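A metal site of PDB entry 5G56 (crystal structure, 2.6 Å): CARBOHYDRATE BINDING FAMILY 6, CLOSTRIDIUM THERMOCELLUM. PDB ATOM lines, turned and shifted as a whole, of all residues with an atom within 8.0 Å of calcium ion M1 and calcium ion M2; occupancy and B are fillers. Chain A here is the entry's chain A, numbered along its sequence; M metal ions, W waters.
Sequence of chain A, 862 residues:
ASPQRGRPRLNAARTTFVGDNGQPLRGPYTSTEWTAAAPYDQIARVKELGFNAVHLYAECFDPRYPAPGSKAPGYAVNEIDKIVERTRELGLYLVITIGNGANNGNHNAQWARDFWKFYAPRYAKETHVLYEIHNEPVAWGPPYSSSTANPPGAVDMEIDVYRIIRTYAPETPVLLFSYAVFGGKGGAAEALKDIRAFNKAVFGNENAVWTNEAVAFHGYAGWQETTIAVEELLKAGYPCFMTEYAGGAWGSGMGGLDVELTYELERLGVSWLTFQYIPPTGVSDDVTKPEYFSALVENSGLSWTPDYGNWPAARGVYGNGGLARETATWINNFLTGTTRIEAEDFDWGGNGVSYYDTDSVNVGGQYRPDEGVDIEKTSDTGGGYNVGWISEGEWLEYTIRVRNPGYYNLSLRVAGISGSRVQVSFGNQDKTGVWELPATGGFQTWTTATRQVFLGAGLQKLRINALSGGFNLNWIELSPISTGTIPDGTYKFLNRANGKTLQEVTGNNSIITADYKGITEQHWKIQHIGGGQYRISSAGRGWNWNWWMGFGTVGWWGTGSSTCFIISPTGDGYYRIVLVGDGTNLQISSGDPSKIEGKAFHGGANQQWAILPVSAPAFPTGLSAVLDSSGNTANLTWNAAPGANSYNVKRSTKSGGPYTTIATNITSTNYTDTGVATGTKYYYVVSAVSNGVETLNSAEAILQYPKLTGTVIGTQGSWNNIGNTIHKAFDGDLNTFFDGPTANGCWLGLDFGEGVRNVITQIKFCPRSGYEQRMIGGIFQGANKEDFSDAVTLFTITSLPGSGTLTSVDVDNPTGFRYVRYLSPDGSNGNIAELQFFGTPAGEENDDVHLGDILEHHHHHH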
ATOM      1  N   ASN A 351      18.960  31.385 -27.107  1.00  0.00           N
ATOM      2  CA  ASN A 351      19.576  30.082 -26.910  1.00  0.00           C
ATOM      3  C   ASN A 351      20.716  30.004 -27.893  1.00  0.00           C
ATOM      4  O   ASN A 351      20.522  30.245 -29.085  1.00  0.00           O
ATOM      5  CB  ASN A 351      18.571  28.944 -27.142  1.00  0.00           C
ATOM      6  CG  ASN A 351      18.844  27.732 -26.271  1.00  0.00           C
ATOM      7  OD1 ASN A 351      19.961  27.526 -25.816  1.00  0.00           O
ATOM      8  ND2 ASN A 351      17.813  26.918 -26.033  1.00  0.00           N
ATOM      9  N   TYR A 355      22.821  32.287 -23.352  1.00  0.00           N
ATOM     10  CA  TYR A 355      22.787  31.043 -22.579  1.00  0.00           C
ATOM     11  C   TYR A 355      22.691  29.886 -23.570  1.00  0.00           C
ATOM     12  O   TYR A 355      22.350  30.112 -24.740  1.00  0.00           O
ATOM     13  CB  TYR A 355      21.591  30.993 -21.602  1.00  0.00           C
ATOM     14  CG  TYR A 355      20.233  30.994 -22.292  1.00  0.00           C
ATOM     15  CD1 TYR A 355      19.593  32.187 -22.613  1.00  0.00           C
ATOM     16  CD2 TYR A 355      19.601  29.794 -22.620  1.00  0.00           C
ATOM     17  CE1 TYR A 355      18.364  32.196 -23.247  1.00  0.00           C
ATOM     18  CE2 TYR A 355      18.374  29.798 -23.270  1.00  0.00           C
ATOM     19  CZ  TYR A 355      17.763  30.990 -23.580  1.00  0.00           C
ATOM     20  OH  TYR A 355      16.533  31.000 -24.214  1.00  0.00           O
ATOM     21  N   TYR A 356      23.012  28.682 -23.122  1.00  0.00           N
ATOM     22  CA  TYR A 356      22.637  27.471 -23.856  1.00  0.00           C
ATOM     23  C   TYR A 356      21.890  26.555 -22.895  1.00  0.00           C
ATOM     24  O   TYR A 356      22.368  26.244 -21.799  1.00  0.00           O
ATOM     25  CB  TYR A 356      23.862  26.767 -24.495  1.00  0.00           C
ATOM     26  CG  TYR A 356      23.532  25.359 -24.977  1.00  0.00           C
ATOM     27  CD1 TYR A 356      22.659  25.145 -26.056  1.00  0.00           C
ATOM     28  CD2 TYR A 356      24.052  24.236 -24.318  1.00  0.00           C
ATOM     29  CE1 TYR A 356      22.335  23.842 -26.471  1.00  0.00           C
ATOM     30  CE2 TYR A 356      23.737  22.946 -24.717  1.00  0.00           C
ATOM     31  CZ  TYR A 356      22.882  22.744 -25.786  1.00  0.00           C
ATOM     32  OH  TYR A 356      22.583  21.445 -26.173  1.00  0.00           O
ATOM     33  N   ASP A 357      20.686  26.153 -23.311  1.00  0.00           N
ATOM     34  CA  ASP A 357      19.890  25.152 -22.620  1.00  0.00           C
ATOM     35  C   ASP A 357      19.467  24.079 -23.625  1.00  0.00           C
ATOM     36  O   ASP A 357      19.258  24.365 -24.810  1.00  0.00           O
ATOM     37  CB  ASP A 357      18.652  25.788 -21.999  1.00  0.00           C
ATOM     38  CG  ASP A 357      18.095  24.976 -20.848  1.00  0.00           C
ATOM     39  OD1 ASP A 357      18.614  25.088 -19.723  1.00  0.00           O
ATOM     40  OD2 ASP A 357      17.143  24.199 -21.043  1.00  0.00           O
ATOM     41  N   THR A 358      19.320  22.845 -23.150  1.00  0.00           N
ATOM     42  CA  THR A 358      19.068  21.682 -24.025  1.00  0.00           C
ATOM     43  C   THR A 358      17.704  21.679 -24.727  1.00  0.00           C
ATOM     44  O   THR A 358      17.524  20.948 -25.694  1.00  0.00           O
ATOM     45  CB  THR A 358      19.279  20.353 -23.287  1.00  0.00           C
ATOM     46  OG1 THR A 358      18.528  20.350 -22.072  1.00  0.00           O
ATOM     47  CG2 THR A 358      20.747  20.161 -22.960  1.00  0.00           C
ATOM     48  N   ASP A 359      16.743  22.476 -24.244  1.00  0.00           N
ATOM     49  CA  ASP A 359      15.474  22.701 -24.963  1.00  0.00           C
ATOM     50  C   ASP A 359      15.022  24.152 -24.849  1.00  0.00           C
ATOM     51  O   ASP A 359      15.576  24.921 -24.057  1.00  0.00           O
ATOM     52  CB  ASP A 359      14.370  21.717 -24.514  1.00  0.00           C
ATOM     53  CG  ASP A 359      14.019  21.836 -23.023  1.00  0.00           C
ATOM     54  OD1 ASP A 359      13.963  22.960 -22.495  1.00  0.00           O
ATOM     55  OD2 ASP A 359      13.772  20.801 -22.369  1.00  0.00           O
ATOM     56  N   SER A 360      14.035  24.511 -25.649  1.00  0.00           N
ATOM     57  CA  SER A 360      13.539  25.887 -25.726  1.00  0.00           C
ATOM     58  C   SER A 360      12.404  26.233 -24.746  1.00  0.00           C
ATOM     59  O   SER A 360      11.922  27.369 -24.741  1.00  0.00           O
ATOM     60  CB  SER A 360      13.090  26.156 -27.167  1.00  0.00           C
ATOM     61  OG  SER A 360      12.066  25.249 -27.535  1.00  0.00           O
ATOM     62  N   VAL A 361      11.964  25.271 -23.927  1.00  0.00           N
ATOM     63  CA  VAL A 361      10.924  25.537 -22.924  1.00  0.00           C
ATOM     64  C   VAL A 361      11.545  25.723 -21.535  1.00  0.00           C
ATOM     65  O   VAL A 361      12.589  25.127 -21.222  1.00  0.00           O
ATOM     66  CB  VAL A 361       9.798  24.453 -22.888  1.00  0.00           C
ATOM     67  CG1 VAL A 361       9.358  24.091 -24.295  1.00  0.00           C
ATOM     68  CG2 VAL A 361      10.227  23.212 -22.128  1.00  0.00           C
ATOM     69  N   ASN A 362      10.895  26.555 -20.722  1.00  0.00           N
ATOM     70  CA  ASN A 362      11.195  26.691 -19.299  1.00  0.00           C
ATOM     71  C   ASN A 362      10.291  25.683 -18.575  1.00  0.00           C
ATOM     72  O   ASN A 362       9.140  25.984 -18.275  1.00  0.00           O
ATOM     73  CB  ASN A 362      10.918  28.134 -18.852  1.00  0.00           C
ATOM     74  CG  ASN A 362      11.163  28.374 -17.372  1.00  0.00           C
ATOM     75  OD1 ASN A 362      11.681  27.520 -16.663  1.00  0.00           O
ATOM     76  ND2 ASN A 362      10.780  29.545 -16.901  1.00  0.00           N
ATOM     77  N   VAL A 363      10.822  24.489 -18.315  1.00  0.00           N
ATOM     78  CA  VAL A 363      10.035  23.409 -17.708  1.00  0.00           C
ATOM     79  C   VAL A 363       9.641  23.703 -16.261  1.00  0.00           C
ATOM     80  O   VAL A 363       8.646  23.173 -15.762  1.00  0.00           O
ATOM     81  CB  VAL A 363      10.727  22.005 -17.772  1.00  0.00           C
ATOM     82  CG1 VAL A 363      11.089  21.637 -19.207  1.00  0.00           C
ATOM     83  CG2 VAL A 363      11.941  21.933 -16.846  1.00  0.00           C
ATOM     84  N   GLY A 364      10.434  24.533 -15.583  1.00  0.00           N
ATOM     85  CA  GLY A 364      10.112  24.995 -14.238  1.00  0.00           C
ATOM     86  C   GLY A 364       8.927  25.945 -14.183  1.00  0.00           C
ATOM     87  O   GLY A 364       8.115  25.883 -13.242  1.00  0.00           O
ATOM     88  N   GLU A 371      11.722  32.027 -22.304  1.00  0.00           N
ATOM     89  CA  GLU A 371      13.113  31.644 -22.538  1.00  0.00           C
ATOM     90  C   GLU A 371      13.391  30.193 -22.167  1.00  0.00           C
ATOM     91  O   GLU A 371      12.636  29.559 -21.418  1.00  0.00           O
ATOM     92  CB  GLU A 371      14.043  32.582 -21.753  1.00  0.00           C
ATOM     93  CG  GLU A 371      14.263  33.926 -22.435  1.00  0.00           C
ATOM     94  CD  GLU A 371      14.779  34.997 -21.511  1.00  0.00           C
ATOM     95  OE1 GLU A 371      13.977  35.531 -20.716  1.00  0.00           O
ATOM     96  OE2 GLU A 371      15.991  35.313 -21.587  1.00  0.00           O
ATOM     97  N   GLY A 372      14.494  29.665 -22.692  1.00  0.00           N
ATOM     98  CA  GLY A 372      14.851  28.258 -22.530  1.00  0.00           C
ATOM     99  C   GLY A 372      15.396  27.802 -21.187  1.00  0.00           C
ATOM    100  O   GLY A 372      15.384  26.596 -20.918  1.00  0.00           O
ATOM    101  N   VAL A 373      15.874  28.715 -20.343  1.00  0.00           N
ATOM    102  CA  VAL A 373      16.482  28.349 -19.041  1.00  0.00           C
ATOM    103  C   VAL A 373      15.390  27.881 -18.070  1.00  0.00           C
ATOM    104  O   VAL A 373      14.270  28.414 -18.077  1.00  0.00           O
ATOM    105  CB  VAL A 373      17.309  29.497 -18.426  1.00  0.00           C
ATOM    106  CG1 VAL A 373      17.925  29.100 -17.083  1.00  0.00           C
ATOM    107  CG2 VAL A 373      18.403  29.951 -19.393  1.00  0.00           C
ATOM    108  N   ASP A 374      15.725  26.893 -17.240  1.00  0.00           N
ATOM    109  CA  ASP A 374      14.749  26.233 -16.391  1.00  0.00           C
ATOM    110  C   ASP A 374      14.782  26.747 -14.947  1.00  0.00           C
ATOM    111  O   ASP A 374      15.761  26.546 -14.229  1.00  0.00           O
ATOM    112  CB  ASP A 374      14.953  24.714 -16.478  1.00  0.00           C
ATOM    113  CG  ASP A 374      14.726  24.193 -17.886  1.00  0.00           C
ATOM    114  OD1 ASP A 374      13.636  24.427 -18.425  1.00  0.00           O
ATOM    115  OD2 ASP A 374      15.654  23.587 -18.483  1.00  0.00           O
ATOM    116  N   ILE A 375      13.699  27.405 -14.557  1.00  0.00           N
ATOM    117  CA  ILE A 375      13.640  28.217 -13.338  1.00  0.00           C
ATOM    118  C   ILE A 375      12.464  27.774 -12.450  1.00  0.00           C
ATOM    119  O   ILE A 375      11.347  27.630 -12.925  1.00  0.00           O
ATOM    120  CB  ILE A 375      13.491  29.706 -13.723  1.00  0.00           C
ATOM    121  CG1 ILE A 375      14.464  30.086 -14.834  1.00  0.00           C
ATOM    122  CG2 ILE A 375      13.715  30.611 -12.509  1.00  0.00           C
ATOM    123  CD1 ILE A 375      14.378  31.520 -15.265  1.00  0.00           C
ATOM    124  N   VAL A 387      17.776  28.572 -10.695  1.00  0.00           N
ATOM    125  CA  VAL A 387      17.947  27.820 -11.945  1.00  0.00           C
ATOM    126  C   VAL A 387      18.099  26.349 -11.578  1.00  0.00           C
ATOM    127  O   VAL A 387      18.973  25.999 -10.782  1.00  0.00           O
ATOM    128  CB  VAL A 387      19.198  28.275 -12.751  1.00  0.00           C
ATOM    129  CG1 VAL A 387      19.465  27.350 -13.943  1.00  0.00           C
ATOM    130  CG2 VAL A 387      19.019  29.713 -13.235  1.00  0.00           C
ATOM    131  N   GLY A 388      17.217  25.510 -12.122  1.00  0.00           N
ATOM    132  CA  GLY A 388      17.307  24.044 -11.993  1.00  0.00           C
ATOM    133  C   GLY A 388      17.343  23.372 -13.346  1.00  0.00           C
ATOM    134  O   GLY A 388      17.411  24.034 -14.379  1.00  0.00           O
ATOM    135  N   TRP A 389      17.287  22.035 -13.349  1.00  0.00           N
ATOM    136  CA  TRP A 389      17.379  21.247 -14.595  1.00  0.00           C
ATOM    137  C   TRP A 389      18.664  21.561 -15.406  1.00  0.00           C
ATOM    138  O   TRP A 389      18.618  21.717 -16.627  1.00  0.00           O
ATOM    139  CB  TRP A 389      16.123  21.431 -15.466  1.00  0.00           C
ATOM    140  CG  TRP A 389      14.856  20.958 -14.823  1.00  0.00           C
ATOM    141  CD1 TRP A 389      14.283  19.730 -14.960  1.00  0.00           C
ATOM    142  CD2 TRP A 389      13.979  21.709 -13.961  1.00  0.00           C
ATOM    143  NE1 TRP A 389      13.119  19.661 -14.254  1.00  0.00           N
ATOM    144  CE2 TRP A 389      12.904  20.855 -13.627  1.00  0.00           C
ATOM    145  CE3 TRP A 389      13.992  23.013 -13.453  1.00  0.00           C
ATOM    146  CZ2 TRP A 389      11.860  21.268 -12.787  1.00  0.00           C
ATOM    147  CZ3 TRP A 389      12.946  23.417 -12.616  1.00  0.00           C
ATOM    148  CH2 TRP A 389      11.897  22.539 -12.294  1.00  0.00           C
ATOM    149  N   ILE A 390      19.790  21.662 -14.702  1.00  0.00           N
ATOM    150  CA  ILE A 390      21.068  22.000 -15.325  1.00  0.00           C
ATOM    151  C   ILE A 390      21.669  20.717 -15.884  1.00  0.00           C
ATOM    152  O   ILE A 390      22.117  19.869 -15.115  1.00  0.00           O
ATOM    153  CB  ILE A 390      22.035  22.678 -14.319  1.00  0.00           C
ATOM    154  CG1 ILE A 390      21.426  23.983 -13.781  1.00  0.00           C
ATOM    155  CG2 ILE A 390      23.389  22.971 -14.965  1.00  0.00           C
ATOM    156  CD1 ILE A 390      22.199  24.612 -12.639  1.00  0.00           C
ATOM    157  N   SER A 391      21.643  20.551 -17.202  1.00  0.00           N
ATOM    158  CA  SER A 391      22.324  19.448 -17.895  1.00  0.00           C
ATOM    159  C   SER A 391      23.753  19.853 -18.245  1.00  0.00           C
ATOM    160  O   SER A 391      24.026  21.049 -18.393  1.00  0.00           O
ATOM    161  CB  SER A 391      21.586  19.047 -19.176  1.00  0.00           C
ATOM    162  OG  SER A 391      20.347  18.438 -18.865  1.00  0.00           O
ATOM    163  N   GLU A 392      24.638  18.863 -18.380  1.00  0.00           N
ATOM    164  CA  GLU A 392      26.033  19.135 -18.737  1.00  0.00           C
ATOM    165  C   GLU A 392      26.109  19.696 -20.149  1.00  0.00           C
ATOM    166  O   GLU A 392      25.294  19.338 -21.002  1.00  0.00           O
ATOM    167  CB  GLU A 392      26.958  17.902 -18.533  1.00  0.00           C
ATOM    168  CG  GLU A 392      27.059  16.884 -19.663  1.00  0.00           C
ATOM    169  CD  GLU A 392      28.125  15.824 -19.379  1.00  0.00           C
ATOM    170  OE1 GLU A 392      27.866  14.888 -18.604  1.00  0.00           O
ATOM    171  OE2 GLU A 392      29.229  15.927 -19.940  1.00  0.00           O
ATOM    172  N   GLU A 394      25.425  22.826 -20.657  1.00  0.00           N
ATOM    173  CA  GLU A 394      24.675  24.073 -20.554  1.00  0.00           C
ATOM    174  C   GLU A 394      25.521  25.179 -19.983  1.00  0.00           C
ATOM    175  O   GLU A 394      26.542  24.930 -19.310  1.00  0.00           O
ATOM    176  CB  GLU A 394      23.394  23.897 -19.730  1.00  0.00           C
ATOM    177  CG  GLU A 394      22.377  23.003 -20.426  1.00  0.00           C
ATOM    178  CD  GLU A 394      21.011  23.037 -19.781  1.00  0.00           C
ATOM    179  OE1 GLU A 394      20.927  23.345 -18.567  1.00  0.00           O
ATOM    180  OE2 GLU A 394      20.016  22.747 -20.465  1.00  0.00           O
ATOM    181  N   TRP A 395      25.111  26.411 -20.252  1.00  0.00           N
ATOM    182  CA  TRP A 395      25.803  27.568 -19.730  1.00  0.00           C
ATOM    183  C   TRP A 395      24.923  28.806 -19.682  1.00  0.00           C
ATOM    184  O   TRP A 395      23.868  28.878 -20.313  1.00  0.00           O
ATOM    185  CB  TRP A 395      27.107  27.833 -20.516  1.00  0.00           C
ATOM    186  CG  TRP A 395      26.991  27.894 -22.025  1.00  0.00           C
ATOM    187  CD1 TRP A 395      27.208  26.868 -22.918  1.00  0.00           C
ATOM    188  CD2 TRP A 395      26.677  29.049 -22.811  1.00  0.00           C
ATOM    189  NE1 TRP A 395      27.027  27.311 -24.202  1.00  0.00           N
ATOM    190  CE2 TRP A 395      26.693  28.642 -24.171  1.00  0.00           C
ATOM    191  CE3 TRP A 395      26.367  30.381 -22.507  1.00  0.00           C
ATOM    192  CZ2 TRP A 395      26.421  29.527 -25.221  1.00  0.00           C
ATOM    193  CZ3 TRP A 395      26.093  31.257 -23.561  1.00  0.00           C
ATOM    194  CH2 TRP A 395      26.127  30.828 -24.904  1.00  0.00           C
ATOM    195  N   LEU A 396      25.378  29.760 -18.867  1.00  0.00           N
ATOM    196  CA  LEU A 396      24.651  30.980 -18.556  1.00  0.00           C
ATOM    197  C   LEU A 396      25.664  32.124 -18.556  1.00  0.00           C
ATOM    198  O   LEU A 396      26.685  32.019 -17.879  1.00  0.00           O
ATOM    199  CB  LEU A 396      23.990  30.842 -17.185  1.00  0.00           C
ATOM    200  CG  LEU A 396      23.009  29.671 -16.981  1.00  0.00           C
ATOM    201  CD1 LEU A 396      22.751  29.385 -15.520  1.00  0.00           C
ATOM    202  CD2 LEU A 396      21.691  29.938 -17.692  1.00  0.00           C
HETATM  203 CA    CA M   1      18.059  23.274 -18.345  1.00  0.00          CA
HETATM  204 CA    CA M   2      14.772  24.214 -20.868  1.00  0.00          CA
HETATM  205  O   HOH W   1      17.442  21.473 -19.806  1.00  0.00           O
HETATM  206  O   HOH W   2      18.415  24.948 -16.810  1.00  0.00           O
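Water W1 lies within hydrogen-bond range of the side-chain hydroxyl of Thr 358 and the side-chain carboxylate of Glu 394. Water W2 lies within hydrogen-bond range of O of Gly 388 (2.8 Å) and N of Asp 374 (3.3 Å).
Five residues have an atom within 4 Å of calcium ion M2: Asp 357, Asp 359, Val 361, Gly 372 and Asp 374. The nearest printed residue that does not touch calcium ion M2 is Asn 362 (4.5 Å).
Calcium ion M1 is bound by water W2. OD1 of Asp 357 is bound to calcium ion M1 (2.3 Å). O of Trp 389 is bound to calcium ion M1, at 2.4 Å. Water W1 binds calcium ion M1 (2.4 Å). OD2 of Asp 374 binds calcium ion M1. Calcium ion M1 is bound by OE1 of Glu 394. Slightly farther from calcium ion M1 lies OE2 of Glu 394 (2.9 Å). Slightly farther from calcium ion M1 lies OD2 of Asp 357 (3.0 Å).
Within 4 Å of calcium ion M1: Asp 357, Asp 374, Trp 389 and Glu 394. The nearest printed residue that does not touch calcium ion M1 is Gly 388 (4.1 Å).
OD1 of Asp 359 binds calcium ion M2, at 2.2 Å. Calcium ion M2 is bound by OD2 of Asp 357 (2.4 Å). Calcium ion M2 is bound by the backbone carbonyl oxygen (O) of Val 361, 2.4 Å away. O of Gly 372 is bound to calcium ion M2, at 2.5 Å. Calcium ion M2 is bound by OD2 of Asp 374, 2.6 Å away. OD1 of Asp 374 is bound to calcium ion M2 (2.7 Å). Calcium ion M2 has six donor atoms within binding distance.
N of Gly 372 sits at hydrogen-bond distance from OH of Tyr 355 (2.9 Å). The side-chain carboxylate (OE1) of Glu 394 lies close to the backbone NH (N) of Ser 391 (3.2 Å). The side-chain carboxylate (OD1) of Asp 374 lies close to the backbone NH (N) of Val 363, at 2.8 Å. The backbone carbonyl oxygen (O) of Asp 374 lies within hydrogen-bond range of the backbone NH (N) of Gly 388 (2.8 Å). The backbone NH (N) of Asp 357 lies within hydrogen-bond range of the side-chain amide oxygen (OD1) of Asn 351, 2.9 Å away. OE2 of Glu 394 sits at hydrogen-bond distance from N of Thr 358, at 2.8 Å.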
